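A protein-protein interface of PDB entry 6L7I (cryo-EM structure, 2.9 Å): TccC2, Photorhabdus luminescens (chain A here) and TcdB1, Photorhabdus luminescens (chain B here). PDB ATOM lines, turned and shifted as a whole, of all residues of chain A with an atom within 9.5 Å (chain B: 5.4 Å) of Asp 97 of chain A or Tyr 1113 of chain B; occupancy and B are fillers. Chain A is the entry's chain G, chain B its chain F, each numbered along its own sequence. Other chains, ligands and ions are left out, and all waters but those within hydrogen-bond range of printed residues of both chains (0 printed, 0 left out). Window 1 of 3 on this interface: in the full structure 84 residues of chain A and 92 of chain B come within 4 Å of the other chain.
Among the printed residues, pairs that only touch across the chains: Asn 76 of chain A with Val 1086 of chain B (3.3 Å), Asn 76 of chain A with Leu 1087 of chain B (3.999 Å), Leu 82 of chain A with Leu 1087 of chain B (3.7 Å), Asp 97 of chain A with Ala 1111 of chain B (3.3 Å), Asp 97 of chain A with Tyr 1113 of chain B (3.6 Å), Asp 97 of chain A with Leu 1155 of chain B (3.8 Å), Ile 98 of chain A with Gly 1112 of chain B (3.4 Å), Ile 98 of chain A with Tyr 1113 of chain B (3.6 Å) and Ile 98 of chain A with Ala 1131 of chain B (3.7 Å).
N of Val 1086 of chain B lies within hydrogen-bond range of O of Trp 1129 of chain B, at 3.0 Å. The backbone carbonyl oxygen of Leu 1087 of chain B is in hydrogen-bond range of the backbone NH of Trp 1129 of chain B, at 2.7 Å. The backbone carbonyl oxygen (O) of Leu 1108 of chain B lies close to the backbone NH (N) of Tyr 1113 of chain B. The backbone NH (N) of Gln 80 of chain A sits at hydrogen-bond distance from the side-chain amide oxygen (OD1) of Asn 76 of chain A (2.7 Å). O of Leu 82 of chain A is in hydrogen-bond range of N of Thr 94 of chain A (3.3 Å). The backbone carbonyl oxygen (O) of Ser 100 of chain A is in hydrogen-bond range of the side-chain amide nitrogen (ND2) of Asn 96 of chain A (3.3 Å).
Printed residues of chain A that touch a printed residue of chain B: Asn 76, Leu 77, Leu 82, Asn 96, Asp 97 and Ile 98. Hydrophobic or aromatic side chains of chain A within 4 Å of the printed part of chain B: Leu 77, Leu 82 and Ile 98. Printed residues of chain B that touch a printed residue of chain A: Val 1086, Leu 1087, Ala 1111, Gly 1112, Tyr 1113, Ala 1131 and Leu 1155. Hydrophobic or aromatic side chains of chain B within 4 Å of the printed part of chain A: Leu 1087, Ala 1111, Tyr 1113, Ala 1131 and Leu 1155. Along chain B the printed residues that touch a printed residue of chain A span positions 1086 to 1155. Among the printed residues, no Asp or Glu carboxylate lies within 4 Å of a Lys or Arg side-chain nitrogen of the other chain.
Asp 97 of chain A touches three residues of chain B. No residue of chain A comes within 4 Å of Leu 1108 of chain B. Of chain A, only Asp 97 and Ile 98 come within 4 Å of Ala 1111 of chain B. Of chain A, only Ile 98 (3.4 Å) comes within 4 Å of Gly 1112 of chain B. Printed residues of chain A within 4 Å of Val 1086 of chain B: Asn 76 (3.3 Å) and Leu 77 (2.9 Å). Of the printed residues of chain B, Asn 96 of chain A touches Tyr 1113 (2.4 Å). Printed residues of chain B within 4 Å of Leu 77 of chain A: Val 1086. Printed residues of chain B within 4 Å of Leu 82 of chain A: Leu 1087. Of the printed residues of chain A, Ala 1131 of chain B touches Ile 98. Leu 104 of chain A touches none of the printed residues of chain B. Glu 118 of chain A touches none of the printed residues of chain B. The nearest residue of chain A that does not touch Tyr 1113 of chain B is Leu 95 of chain A (4.2 Å).
The backbone carbonyl oxygen (O) of Val 1086 of chain B lies within hydrogen-bond range of the backbone NH (N) of Leu 77 of chain A, 2.9 Å away. The backbone carbonyl oxygen of Ala 1111 of chain B lies close to the backbone NH of Ile 98 of chain A, 3.4 Å away. O of Asn 96 of chain A lies close to OH of Tyr 1113 of chain B (2.4 Å).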
ATOM      1  N   ASN A  76       7.325 -12.901  17.228  1.00  0.00           N
ATOM      2  CA  ASN A  76       7.925 -14.075  16.616  1.00  0.00           C
ATOM      3  C   ASN A  76       6.894 -14.724  15.695  1.00  0.00           C
ATOM      4  O   ASN A  76       5.864 -14.134  15.370  1.00  0.00           O
ATOM      5  CB  ASN A  76       8.473 -15.023  17.681  1.00  0.00           C
ATOM      6  CG  ASN A  76       7.407 -15.575  18.584  1.00  0.00           C
ATOM      7  OD1 ASN A  76       6.365 -14.968  18.770  1.00  0.00           O
ATOM      8  ND2 ASN A  76       7.671 -16.733  19.163  1.00  0.00           N
ATOM      9  N   LEU A  77       7.166 -15.943  15.242  1.00  0.00           N
ATOM     10  CA  LEU A  77       6.240 -16.607  14.338  1.00  0.00           C
ATOM     11  C   LEU A  77       5.015 -17.165  15.046  1.00  0.00           C
ATOM     12  O   LEU A  77       4.040 -17.515  14.374  1.00  0.00           O
ATOM     13  CB  LEU A  77       6.958 -17.722  13.574  1.00  0.00           C
ATOM     14  CG  LEU A  77       8.143 -17.310  12.695  1.00  0.00           C
ATOM     15  CD1 LEU A  77       8.625 -18.468  11.862  1.00  0.00           C
ATOM     16  CD2 LEU A  77       7.794 -16.144  11.802  1.00  0.00           C
ATOM     17  N   ALA A  78       5.025 -17.245  16.373  1.00  0.00           N
ATOM     18  CA  ALA A  78       3.868 -17.720  17.114  1.00  0.00           C
ATOM     19  C   ALA A  78       2.955 -16.596  17.579  1.00  0.00           C
ATOM     20  O   ALA A  78       1.818 -16.867  17.977  1.00  0.00           O
ATOM     21  CB  ALA A  78       4.314 -18.540  18.321  1.00  0.00           C
ATOM     22  N   GLN A  80       4.043 -14.054  19.905  1.00  0.00           N
ATOM     23  CA  GLN A  80       4.472 -13.504  21.179  1.00  0.00           C
ATOM     24  C   GLN A  80       5.430 -12.344  20.954  1.00  0.00           C
ATOM     25  O   GLN A  80       6.216 -12.341  20.007  1.00  0.00           O
ATOM     26  CB  GLN A  80       5.146 -14.577  22.029  1.00  0.00           C
ATOM     27  CG  GLN A  80       4.510 -15.941  21.919  1.00  0.00           C
ATOM     28  CD  GLN A  80       5.460 -17.047  22.316  1.00  0.00           C
ATOM     29  OE1 GLN A  80       5.882 -17.134  23.466  1.00  0.00           O
ATOM     30  NE2 GLN A  80       5.811 -17.896  21.362  1.00  0.00           N
ATOM     31  N   VAL A  81       5.368 -11.362  21.843  1.00  0.00           N
ATOM     32  CA  VAL A  81       6.120 -10.127  21.667  1.00  0.00           C
ATOM     33  C   VAL A  81       7.578 -10.366  22.037  1.00  0.00           C
ATOM     34  O   VAL A  81       7.881 -10.854  23.129  1.00  0.00           O
ATOM     35  CB  VAL A  81       5.515  -9.000  22.514  1.00  0.00           C
ATOM     36  CG1 VAL A  81       6.243  -7.712  22.266  1.00  0.00           C
ATOM     37  CG2 VAL A  81       4.058  -8.840  22.214  1.00  0.00           C
ATOM     38  N   LEU A  82       8.485 -10.029  21.118  1.00  0.00           N
ATOM     39  CA  LEU A  82       9.914 -10.083  21.385  1.00  0.00           C
ATOM     40  C   LEU A  82      10.515  -8.723  21.676  1.00  0.00           C
ATOM     41  O   LEU A  82      11.585  -8.655  22.285  1.00  0.00           O
ATOM     42  CB  LEU A  82      10.661 -10.684  20.197  1.00  0.00           C
ATOM     43  CG  LEU A  82      10.208 -12.028  19.665  1.00  0.00           C
ATOM     44  CD1 LEU A  82      10.908 -12.268  18.359  1.00  0.00           C
ATOM     45  CD2 LEU A  82      10.533 -13.112  20.658  1.00  0.00           C
ATOM     46  N   THR A  94      11.984  -9.362  25.442  1.00  0.00           N
ATOM     47  CA  THR A  94      11.517 -10.537  26.162  1.00  0.00           C
ATOM     48  C   THR A  94      11.866 -11.781  25.360  1.00  0.00           C
ATOM     49  O   THR A  94      11.630 -11.826  24.152  1.00  0.00           O
ATOM     50  CB  THR A  94      10.000 -10.469  26.399  1.00  0.00           C
ATOM     51  OG1 THR A  94       9.668  -9.242  27.057  1.00  0.00           O
ATOM     52  CG2 THR A  94       9.538 -11.611  27.277  1.00  0.00           C
ATOM     53  N   LEU A  95      12.436 -12.780  26.026  1.00  0.00           N
ATOM     54  CA  LEU A  95      12.670 -14.084  25.428  1.00  0.00           C
ATOM     55  C   LEU A  95      12.048 -15.158  26.304  1.00  0.00           C
ATOM     56  O   LEU A  95      12.268 -15.176  27.518  1.00  0.00           O
ATOM     57  CB  LEU A  95      14.160 -14.357  25.244  1.00  0.00           C
ATOM     58  CG  LEU A  95      14.487 -15.744  24.688  1.00  0.00           C
ATOM     59  CD1 LEU A  95      13.856 -15.944  23.322  1.00  0.00           C
ATOM     60  CD2 LEU A  95      15.968 -15.949  24.606  1.00  0.00           C
ATOM     61  N   ASN A  96      11.263 -16.038  25.689  1.00  0.00           N
ATOM     62  CA  ASN A  96      10.699 -17.204  26.347  1.00  0.00           C
ATOM     63  C   ASN A  96      11.284 -18.464  25.726  1.00  0.00           C
ATOM     64  O   ASN A  96      11.728 -18.454  24.577  1.00  0.00           O
ATOM     65  CB  ASN A  96       9.178 -17.241  26.219  1.00  0.00           C
ATOM     66  CG  ASN A  96       8.498 -16.165  27.021  1.00  0.00           C
ATOM     67  OD1 ASN A  96       9.085 -15.133  27.323  1.00  0.00           O
ATOM     68  ND2 ASN A  96       7.245 -16.402  27.373  1.00  0.00           N
ATOM     69  N   ASP A  97      11.276 -19.552  26.489  1.00  0.00           N
ATOM     70  CA  ASP A  97      11.785 -20.826  26.000  1.00  0.00           C
ATOM     71  C   ASP A  97      10.676 -21.595  25.290  1.00  0.00           C
ATOM     72  O   ASP A  97       9.635 -21.042  24.925  1.00  0.00           O
ATOM     73  CB  ASP A  97      12.403 -21.643  27.130  1.00  0.00           C
ATOM     74  CG  ASP A  97      11.465 -21.851  28.295  1.00  0.00           C
ATOM     75  OD1 ASP A  97      11.707 -21.247  29.354  1.00  0.00           O
ATOM     76  OD2 ASP A  97      10.505 -22.636  28.175  1.00  0.00           O
ATOM     77  N   ILE A  98      10.921 -22.890  25.067  1.00  0.00           N
ATOM     78  CA  ILE A  98       9.975 -23.788  24.415  1.00  0.00           C
ATOM     79  C   ILE A  98       8.668 -23.908  25.182  1.00  0.00           C
ATOM     80  O   ILE A  98       7.595 -23.974  24.574  1.00  0.00           O
ATOM     81  CB  ILE A  98      10.629 -25.172  24.236  1.00  0.00           C
ATOM     82  CG1 ILE A  98      11.981 -25.029  23.567  1.00  0.00           C
ATOM     83  CG2 ILE A  98       9.778 -26.085  23.391  1.00  0.00           C
ATOM     84  CD1 ILE A  98      11.908 -24.436  22.213  1.00  0.00           C
ATOM     85  N   GLU A  99       8.723 -23.911  26.510  1.00  0.00           N
ATOM     86  CA  GLU A  99       7.541 -24.104  27.340  1.00  0.00           C
ATOM     87  C   GLU A  99       6.895 -22.782  27.738  1.00  0.00           C
ATOM     88  O   GLU A  99       6.122 -22.736  28.696  1.00  0.00           O
ATOM     89  CB  GLU A  99       7.901 -24.924  28.570  1.00  0.00           C
ATOM     90  CG  GLU A  99       8.846 -26.048  28.249  1.00  0.00           C
ATOM     91  CD  GLU A  99       8.672 -27.223  29.169  1.00  0.00           C
ATOM     92  OE1 GLU A  99       7.885 -27.107  30.130  1.00  0.00           O
ATOM     93  OE2 GLU A  99       9.306 -28.269  28.924  1.00  0.00           O
ATOM     94  N   SER A 100       7.229 -21.711  27.010  1.00  0.00           N
ATOM     95  CA  SER A 100       6.685 -20.359  27.190  1.00  0.00           C
ATOM     96  C   SER A 100       6.940 -19.815  28.593  1.00  0.00           C
ATOM     97  O   SER A 100       6.162 -19.026  29.128  1.00  0.00           O
ATOM     98  CB  SER A 100       5.196 -20.303  26.840  1.00  0.00           C
ATOM     99  OG  SER A 100       5.008 -20.298  25.434  1.00  0.00           O
ATOM    100  N   ARG A 101       8.043 -20.241  29.192  1.00  0.00           N
ATOM    101  CA  ARG A 101       8.486 -19.685  30.456  1.00  0.00           C
ATOM    102  C   ARG A 101       9.503 -18.586  30.200  1.00  0.00           C
ATOM    103  O   ARG A 101      10.287 -18.688  29.256  1.00  0.00           O
ATOM    104  CB  ARG A 101       9.116 -20.762  31.335  1.00  0.00           C
ATOM    105  CG  ARG A 101       8.355 -22.060  31.373  1.00  0.00           C
ATOM    106  CD  ARG A 101       9.153 -23.135  32.080  1.00  0.00           C
ATOM    107  NE  ARG A 101      10.477 -23.306  31.500  1.00  0.00           N
ATOM    108  CZ  ARG A 101      11.303 -24.295  31.812  1.00  0.00           C
ATOM    109  NH1 ARG A 101      10.941 -25.200  32.703  1.00  0.00           N
ATOM    110  NH2 ARG A 101      12.491 -24.382  31.237  1.00  0.00           N
ATOM    111  N   PRO A 102       9.505 -17.515  30.993  1.00  0.00           N
ATOM    112  CA  PRO A 102      10.434 -16.409  30.732  1.00  0.00           C
ATOM    113  C   PRO A 102      11.869 -16.813  31.029  1.00  0.00           C
ATOM    114  O   PRO A 102      12.147 -17.471  32.030  1.00  0.00           O
ATOM    115  CB  PRO A 102       9.946 -15.307  31.677  1.00  0.00           C
ATOM    116  CG  PRO A 102       8.539 -15.668  31.984  1.00  0.00           C
ATOM    117  CD  PRO A 102       8.517 -17.155  32.020  1.00  0.00           C
ATOM    118  N   VAL A 103      12.772 -16.444  30.121  1.00  0.00           N
ATOM    119  CA  VAL A 103      14.194 -16.746  30.235  1.00  0.00           C
ATOM    120  C   VAL A 103      15.014 -15.477  30.389  1.00  0.00           C
ATOM    121  O   VAL A 103      15.941 -15.417  31.200  1.00  0.00           O
ATOM    122  CB  VAL A 103      14.697 -17.559  29.022  1.00  0.00           C
ATOM    123  CG1 VAL A 103      16.033 -18.200  29.328  1.00  0.00           C
ATOM    124  CG2 VAL A 103      13.708 -18.592  28.640  1.00  0.00           C
ATOM    125  N   LEU A 104      14.695 -14.453  29.604  1.00  0.00           N
ATOM    126  CA  LEU A 104      15.507 -13.249  29.537  1.00  0.00           C
ATOM    127  C   LEU A 104      14.599 -12.060  29.291  1.00  0.00           C
ATOM    128  O   LEU A 104      13.959 -11.977  28.241  1.00  0.00           O
ATOM    129  CB  LEU A 104      16.551 -13.364  28.429  1.00  0.00           C
ATOM    130  CG  LEU A 104      17.812 -12.548  28.652  1.00  0.00           C
ATOM    131  CD1 LEU A 104      18.487 -13.036  29.901  1.00  0.00           C
ATOM    132  CD2 LEU A 104      18.729 -12.726  27.489  1.00  0.00           C
ATOM    133  N   HIS A 115      15.879 -16.080  34.533  1.00  0.00           N
ATOM    134  CA  HIS A 115      15.124 -17.079  35.281  1.00  0.00           C
ATOM    135  C   HIS A 115      15.748 -18.430  34.974  1.00  0.00           C
ATOM    136  O   HIS A 115      15.541 -18.966  33.884  1.00  0.00           O
ATOM    137  CB  HIS A 115      13.640 -17.100  34.910  1.00  0.00           C
ATOM    138  CG  HIS A 115      12.977 -15.757  34.885  1.00  0.00           C
ATOM    139  ND1 HIS A 115      12.122 -15.334  35.877  1.00  0.00           N
ATOM    140  CD2 HIS A 115      13.003 -14.765  33.966  1.00  0.00           C
ATOM    141  CE1 HIS A 115      11.671 -14.129  35.584  1.00  0.00           C
ATOM    142  NE2 HIS A 115      12.194 -13.759  34.430  1.00  0.00           N
ATOM    143  N   ARG A 116      16.506 -18.982  35.911  1.00  0.00           N
ATOM    144  CA  ARG A 116      17.020 -20.332  35.750  1.00  0.00           C
ATOM    145  C   ARG A 116      16.096 -21.314  36.454  1.00  0.00           C
ATOM    146  O   ARG A 116      15.576 -21.032  37.536  1.00  0.00           O
ATOM    147  CB  ARG A 116      18.450 -20.465  36.273  1.00  0.00           C
ATOM    148  CG  ARG A 116      18.675 -20.015  37.688  1.00  0.00           C
ATOM    149  CD  ARG A 116      20.057 -20.437  38.175  1.00  0.00           C
ATOM    150  NE  ARG A 116      20.135 -21.869  38.435  1.00  0.00           N
ATOM    151  CZ  ARG A 116      20.053 -22.413  39.644  1.00  0.00           C
ATOM    152  NH1 ARG A 116      20.131 -23.725  39.788  1.00  0.00           N
ATOM    153  NH2 ARG A 116      19.893 -21.643  40.708  1.00  0.00           N
ATOM    154  N   TYR A 117      15.881 -22.456  35.820  1.00  0.00           N
ATOM    155  CA  TYR A 117      14.915 -23.448  36.256  1.00  0.00           C
ATOM    156  C   TYR A 117      15.644 -24.726  36.666  1.00  0.00           C
ATOM    157  O   TYR A 117      16.873 -24.790  36.682  1.00  0.00           O
ATOM    158  CB  TYR A 117      13.897 -23.712  35.148  1.00  0.00           C
ATOM    159  CG  TYR A 117      13.079 -22.506  34.764  1.00  0.00           C
ATOM    160  CD1 TYR A 117      11.884 -22.232  35.396  1.00  0.00           C
ATOM    161  CD2 TYR A 117      13.496 -21.648  33.762  1.00  0.00           C
ATOM    162  CE1 TYR A 117      11.133 -21.137  35.052  1.00  0.00           C
ATOM    163  CE2 TYR A 117      12.748 -20.551  33.412  1.00  0.00           C
ATOM    164  CZ  TYR A 117      11.571 -20.305  34.063  1.00  0.00           C
ATOM    165  OH  TYR A 117      10.824 -19.213  33.720  1.00  0.00           O
ATOM    166  N   GLU A 118      14.866 -25.746  37.009  1.00  0.00           N
ATOM    167  CA  GLU A 118      15.429 -27.049  37.306  1.00  0.00           C
ATOM    168  C   GLU A 118      15.877 -27.736  36.019  1.00  0.00           C
ATOM    169  O   GLU A 118      15.438 -27.399  34.920  1.00  0.00           O
ATOM    170  CB  GLU A 118      14.404 -27.911  38.037  1.00  0.00           C
ATOM    171  CG  GLU A 118      13.920 -27.344  39.359  1.00  0.00           C
ATOM    172  CD  GLU A 118      12.926 -28.247  40.062  1.00  0.00           C
ATOM    173  OE1 GLU A 118      12.255 -29.043  39.384  1.00  0.00           O
ATOM    174  OE2 GLU A 118      12.815 -28.166  41.298  1.00  0.00           O
ATOM    175  N   GLY A 124      11.234 -29.014  36.185  1.00  0.00           N
ATOM    176  CA  GLY A 124      11.443 -27.720  35.575  1.00  0.00           C
ATOM    177  C   GLY A 124      10.704 -26.603  36.273  1.00  0.00           C
ATOM    178  O   GLY A 124      10.104 -25.743  35.624  1.00  0.00           O
ATOM    179  N   LEU A 126      10.739 -23.224  38.909  1.00  0.00           N
ATOM    180  CA  LEU A 126      11.613 -22.061  38.998  1.00  0.00           C
ATOM    181  C   LEU A 126      12.510 -22.156  40.223  1.00  0.00           C
ATOM    182  O   LEU A 126      12.058 -22.510  41.313  1.00  0.00           O
ATOM    183  CB  LEU A 126      10.787 -20.777  39.048  1.00  0.00           C
ATOM    184  CG  LEU A 126      11.525 -19.438  39.146  1.00  0.00           C
ATOM    185  CD1 LEU A 126      12.455 -19.237  37.974  1.00  0.00           C
ATOM    186  CD2 LEU A 126      10.547 -18.293  39.234  1.00  0.00           C
ATOM    187  N   VAL B1086       9.640 -21.085  15.173  1.00  0.00           N
ATOM    188  CA  VAL B1086       9.163 -19.946  15.951  1.00  0.00           C
ATOM    189  C   VAL B1086       9.996 -18.697  15.702  1.00  0.00           C
ATOM    190  O   VAL B1086       9.503 -17.579  15.865  1.00  0.00           O
ATOM    191  CB  VAL B1086       9.133 -20.282  17.451  1.00  0.00           C
ATOM    192  CG1 VAL B1086       7.945 -21.155  17.772  1.00  0.00           C
ATOM    193  CG2 VAL B1086      10.392 -20.983  17.843  1.00  0.00           C
ATOM    194  N   LEU B1087      11.256 -18.861  15.311  1.00  0.00           N
ATOM    195  CA  LEU B1087      12.132 -17.721  15.076  1.00  0.00           C
ATOM    196  C   LEU B1087      12.922 -17.936  13.798  1.00  0.00           C
ATOM    197  O   LEU B1087      13.405 -19.039  13.541  1.00  0.00           O
ATOM    198  CB  LEU B1087      13.112 -17.503  16.232  1.00  0.00           C
ATOM    199  CG  LEU B1087      12.584 -17.064  17.594  1.00  0.00           C
ATOM    200  CD1 LEU B1087      13.533 -17.510  18.669  1.00  0.00           C
ATOM    201  CD2 LEU B1087      12.433 -15.575  17.637  1.00  0.00           C
ATOM    202  N   LEU B1108      19.878 -18.944  22.732  1.00  0.00           N
ATOM    203  CA  LEU B1108      18.748 -19.593  22.077  1.00  0.00           C
ATOM    204  C   LEU B1108      18.821 -21.110  22.197  1.00  0.00           C
ATOM    205  O   LEU B1108      17.803 -21.764  22.437  1.00  0.00           O
ATOM    206  CB  LEU B1108      18.684 -19.177  20.611  1.00  0.00           C
ATOM    207  CG  LEU B1108      18.093 -17.798  20.334  1.00  0.00           C
ATOM    208  CD1 LEU B1108      18.020 -17.544  18.849  1.00  0.00           C
ATOM    209  CD2 LEU B1108      16.727 -17.686  20.953  1.00  0.00           C
ATOM    210  N   THR B1109      20.010 -21.691  22.055  1.00  0.00           N
ATOM    211  CA  THR B1109      20.114 -23.137  22.185  1.00  0.00           C
ATOM    212  C   THR B1109      20.048 -23.590  23.636  1.00  0.00           C
ATOM    213  O   THR B1109      19.848 -24.782  23.887  1.00  0.00           O
ATOM    214  CB  THR B1109      21.400 -23.646  21.532  1.00  0.00           C
ATOM    215  OG1 THR B1109      21.350 -25.071  21.433  1.00  0.00           O
ATOM    216  CG2 THR B1109      22.609 -23.273  22.353  1.00  0.00           C
ATOM    217  N   ALA B1111      17.709 -22.217  25.616  1.00  0.00           N
ATOM    218  CA  ALA B1111      16.270 -22.164  25.809  1.00  0.00           C
ATOM    219  C   ALA B1111      15.530 -23.254  25.049  1.00  0.00           C
ATOM    220  O   ALA B1111      14.303 -23.205  24.976  1.00  0.00           O
ATOM    221  CB  ALA B1111      15.734 -20.792  25.401  1.00  0.00           C
ATOM    222  N   GLY B1112      16.238 -24.222  24.475  1.00  0.00           N
ATOM    223  CA  GLY B1112      15.623 -25.365  23.843  1.00  0.00           C
ATOM    224  C   GLY B1112      15.395 -25.238  22.354  1.00  0.00           C
ATOM    225  O   GLY B1112      14.802 -26.145  21.762  1.00  0.00           O
ATOM    226  N   TYR B1113      15.825 -24.147  21.733  1.00  0.00           N
ATOM    227  CA  TYR B1113      15.658 -23.989  20.298  1.00  0.00           C
ATOM    228  C   TYR B1113      16.742 -24.749  19.544  1.00  0.00           C
ATOM    229  O   TYR B1113      17.842 -24.971  20.051  1.00  0.00           O
ATOM    230  CB  TYR B1113      15.690 -22.510  19.916  1.00  0.00           C
ATOM    231  CG  TYR B1113      14.618 -21.688  20.585  1.00  0.00           C
ATOM    232  CD1 TYR B1113      13.293 -21.811  20.216  1.00  0.00           C
ATOM    233  CD2 TYR B1113      14.932 -20.789  21.588  1.00  0.00           C
ATOM    234  CE1 TYR B1113      12.311 -21.066  20.837  1.00  0.00           C
ATOM    235  CE2 TYR B1113      13.958 -20.036  22.206  1.00  0.00           C
ATOM    236  CZ  TYR B1113      12.653 -20.180  21.825  1.00  0.00           C
ATOM    237  OH  TYR B1113      11.678 -19.435  22.435  1.00  0.00           O
ATOM    238  N   GLN B1114      16.405 -25.177  18.330  1.00  0.00           N
ATOM    239  CA  GLN B1114      17.330 -25.860  17.440  1.00  0.00           C
ATOM    240  C   GLN B1114      17.257 -25.228  16.064  1.00  0.00           C
ATOM    241  O   GLN B1114      16.248 -24.631  15.690  1.00  0.00           O
ATOM    242  CB  GLN B1114      17.022 -27.350  17.302  1.00  0.00           C
ATOM    243  CG  GLN B1114      16.931 -28.098  18.594  1.00  0.00           C
ATOM    244  CD  GLN B1114      15.961 -29.229  18.510  1.00  0.00           C
ATOM    245  OE1 GLN B1114      15.729 -29.776  17.437  1.00  0.00           O
ATOM    246  NE2 GLN B1114      15.377 -29.591  19.642  1.00  0.00           N
ATOM    247  N   GLN B1115      18.328 -25.388  15.302  1.00  0.00           N
ATOM    248  CA  GLN B1115      18.414 -24.854  13.951  1.00  0.00           C
ATOM    249  C   GLN B1115      18.172 -25.988  12.966  1.00  0.00           C
ATOM    250  O   GLN B1115      18.999 -26.895  12.838  1.00  0.00           O
ATOM    251  CB  GLN B1115      19.771 -24.205  13.714  1.00  0.00           C
ATOM    252  CG  GLN B1115      19.766 -22.712  13.857  1.00  0.00           C
ATOM    253  CD  GLN B1115      21.032 -22.091  13.343  1.00  0.00           C
ATOM    254  OE1 GLN B1115      22.113 -22.654  13.491  1.00  0.00           O
ATOM    255  NE2 GLN B1115      20.913 -20.922  12.731  1.00  0.00           N
ATOM    256  N   TRP B1129      14.872 -21.274  13.538  1.00  0.00           N
ATOM    257  CA  TRP B1129      14.942 -21.702  14.931  1.00  0.00           C
ATOM    258  C   TRP B1129      13.594 -22.304  15.305  1.00  0.00           C
ATOM    259  O   TRP B1129      12.592 -21.591  15.387  1.00  0.00           O
ATOM    260  CB  TRP B1129      15.298 -20.536  15.844  1.00  0.00           C
ATOM    261  CG  TRP B1129      16.719 -20.097  15.748  1.00  0.00           C
ATOM    262  CD1 TRP B1129      17.202 -19.045  15.032  1.00  0.00           C
ATOM    263  CD2 TRP B1129      17.846 -20.692  16.395  1.00  0.00           C
ATOM    264  NE1 TRP B1129      18.557 -18.948  15.192  1.00  0.00           N
ATOM    265  CE2 TRP B1129      18.978 -19.947  16.027  1.00  0.00           C
ATOM    266  CE3 TRP B1129      18.007 -21.783  17.250  1.00  0.00           C
ATOM    267  CZ2 TRP B1129      20.252 -20.260  16.484  1.00  0.00           C
ATOM    268  CZ3 TRP B1129      19.272 -22.089  17.703  1.00  0.00           C
ATOM    269  CH2 TRP B1129      20.375 -21.335  17.318  1.00  0.00           C
ATOM    270  N   VAL B1130      13.567 -23.610  15.531  1.00  0.00           N
ATOM    271  CA  VAL B1130      12.326 -24.332  15.723  1.00  0.00           C
ATOM    272  C   VAL B1130      12.103 -24.585  17.204  1.00  0.00           C
ATOM    273  O   VAL B1130      12.999 -24.434  18.036  1.00  0.00           O
ATOM    274  CB  VAL B1130      12.315 -25.658  14.939  1.00  0.00           C
ATOM    275  CG1 VAL B1130      12.384 -25.396  13.457  1.00  0.00           C
ATOM    276  CG2 VAL B1130      13.467 -26.509  15.377  1.00  0.00           C
ATOM    277  N   ALA B1131      10.880 -24.985  17.538  1.00  0.00           N
ATOM    278  CA  ALA B1131      10.494 -25.352  18.897  1.00  0.00           C
ATOM    279  C   ALA B1131      10.074 -26.814  18.872  1.00  0.00           C
ATOM    280  O   ALA B1131       8.918 -27.131  18.581  1.00  0.00           O
ATOM    281  CB  ALA B1131       9.371 -24.463  19.411  1.00  0.00           C
ATOM    282  N   LEU B1155      13.559 -29.714  27.878  1.00  0.00           N
ATOM    283  CA  LEU B1155      13.950 -28.852  28.983  1.00  0.00           C
ATOM    284  C   LEU B1155      13.450 -29.353  30.325  1.00  0.00           C
ATOM    285  O   LEU B1155      14.154 -29.215  31.330  1.00  0.00           O
ATOM    286  CB  LEU B1155      13.420 -27.436  28.762  1.00  0.00           C
ATOM    287  CG  LEU B1155      13.810 -26.732  27.472  1.00  0.00           C
ATOM    288  CD1 LEU B1155      13.099 -25.411  27.396  1.00  0.00           C
ATOM    289  CD2 LEU B1155      15.303 -26.539  27.419  1.00  0.00           C
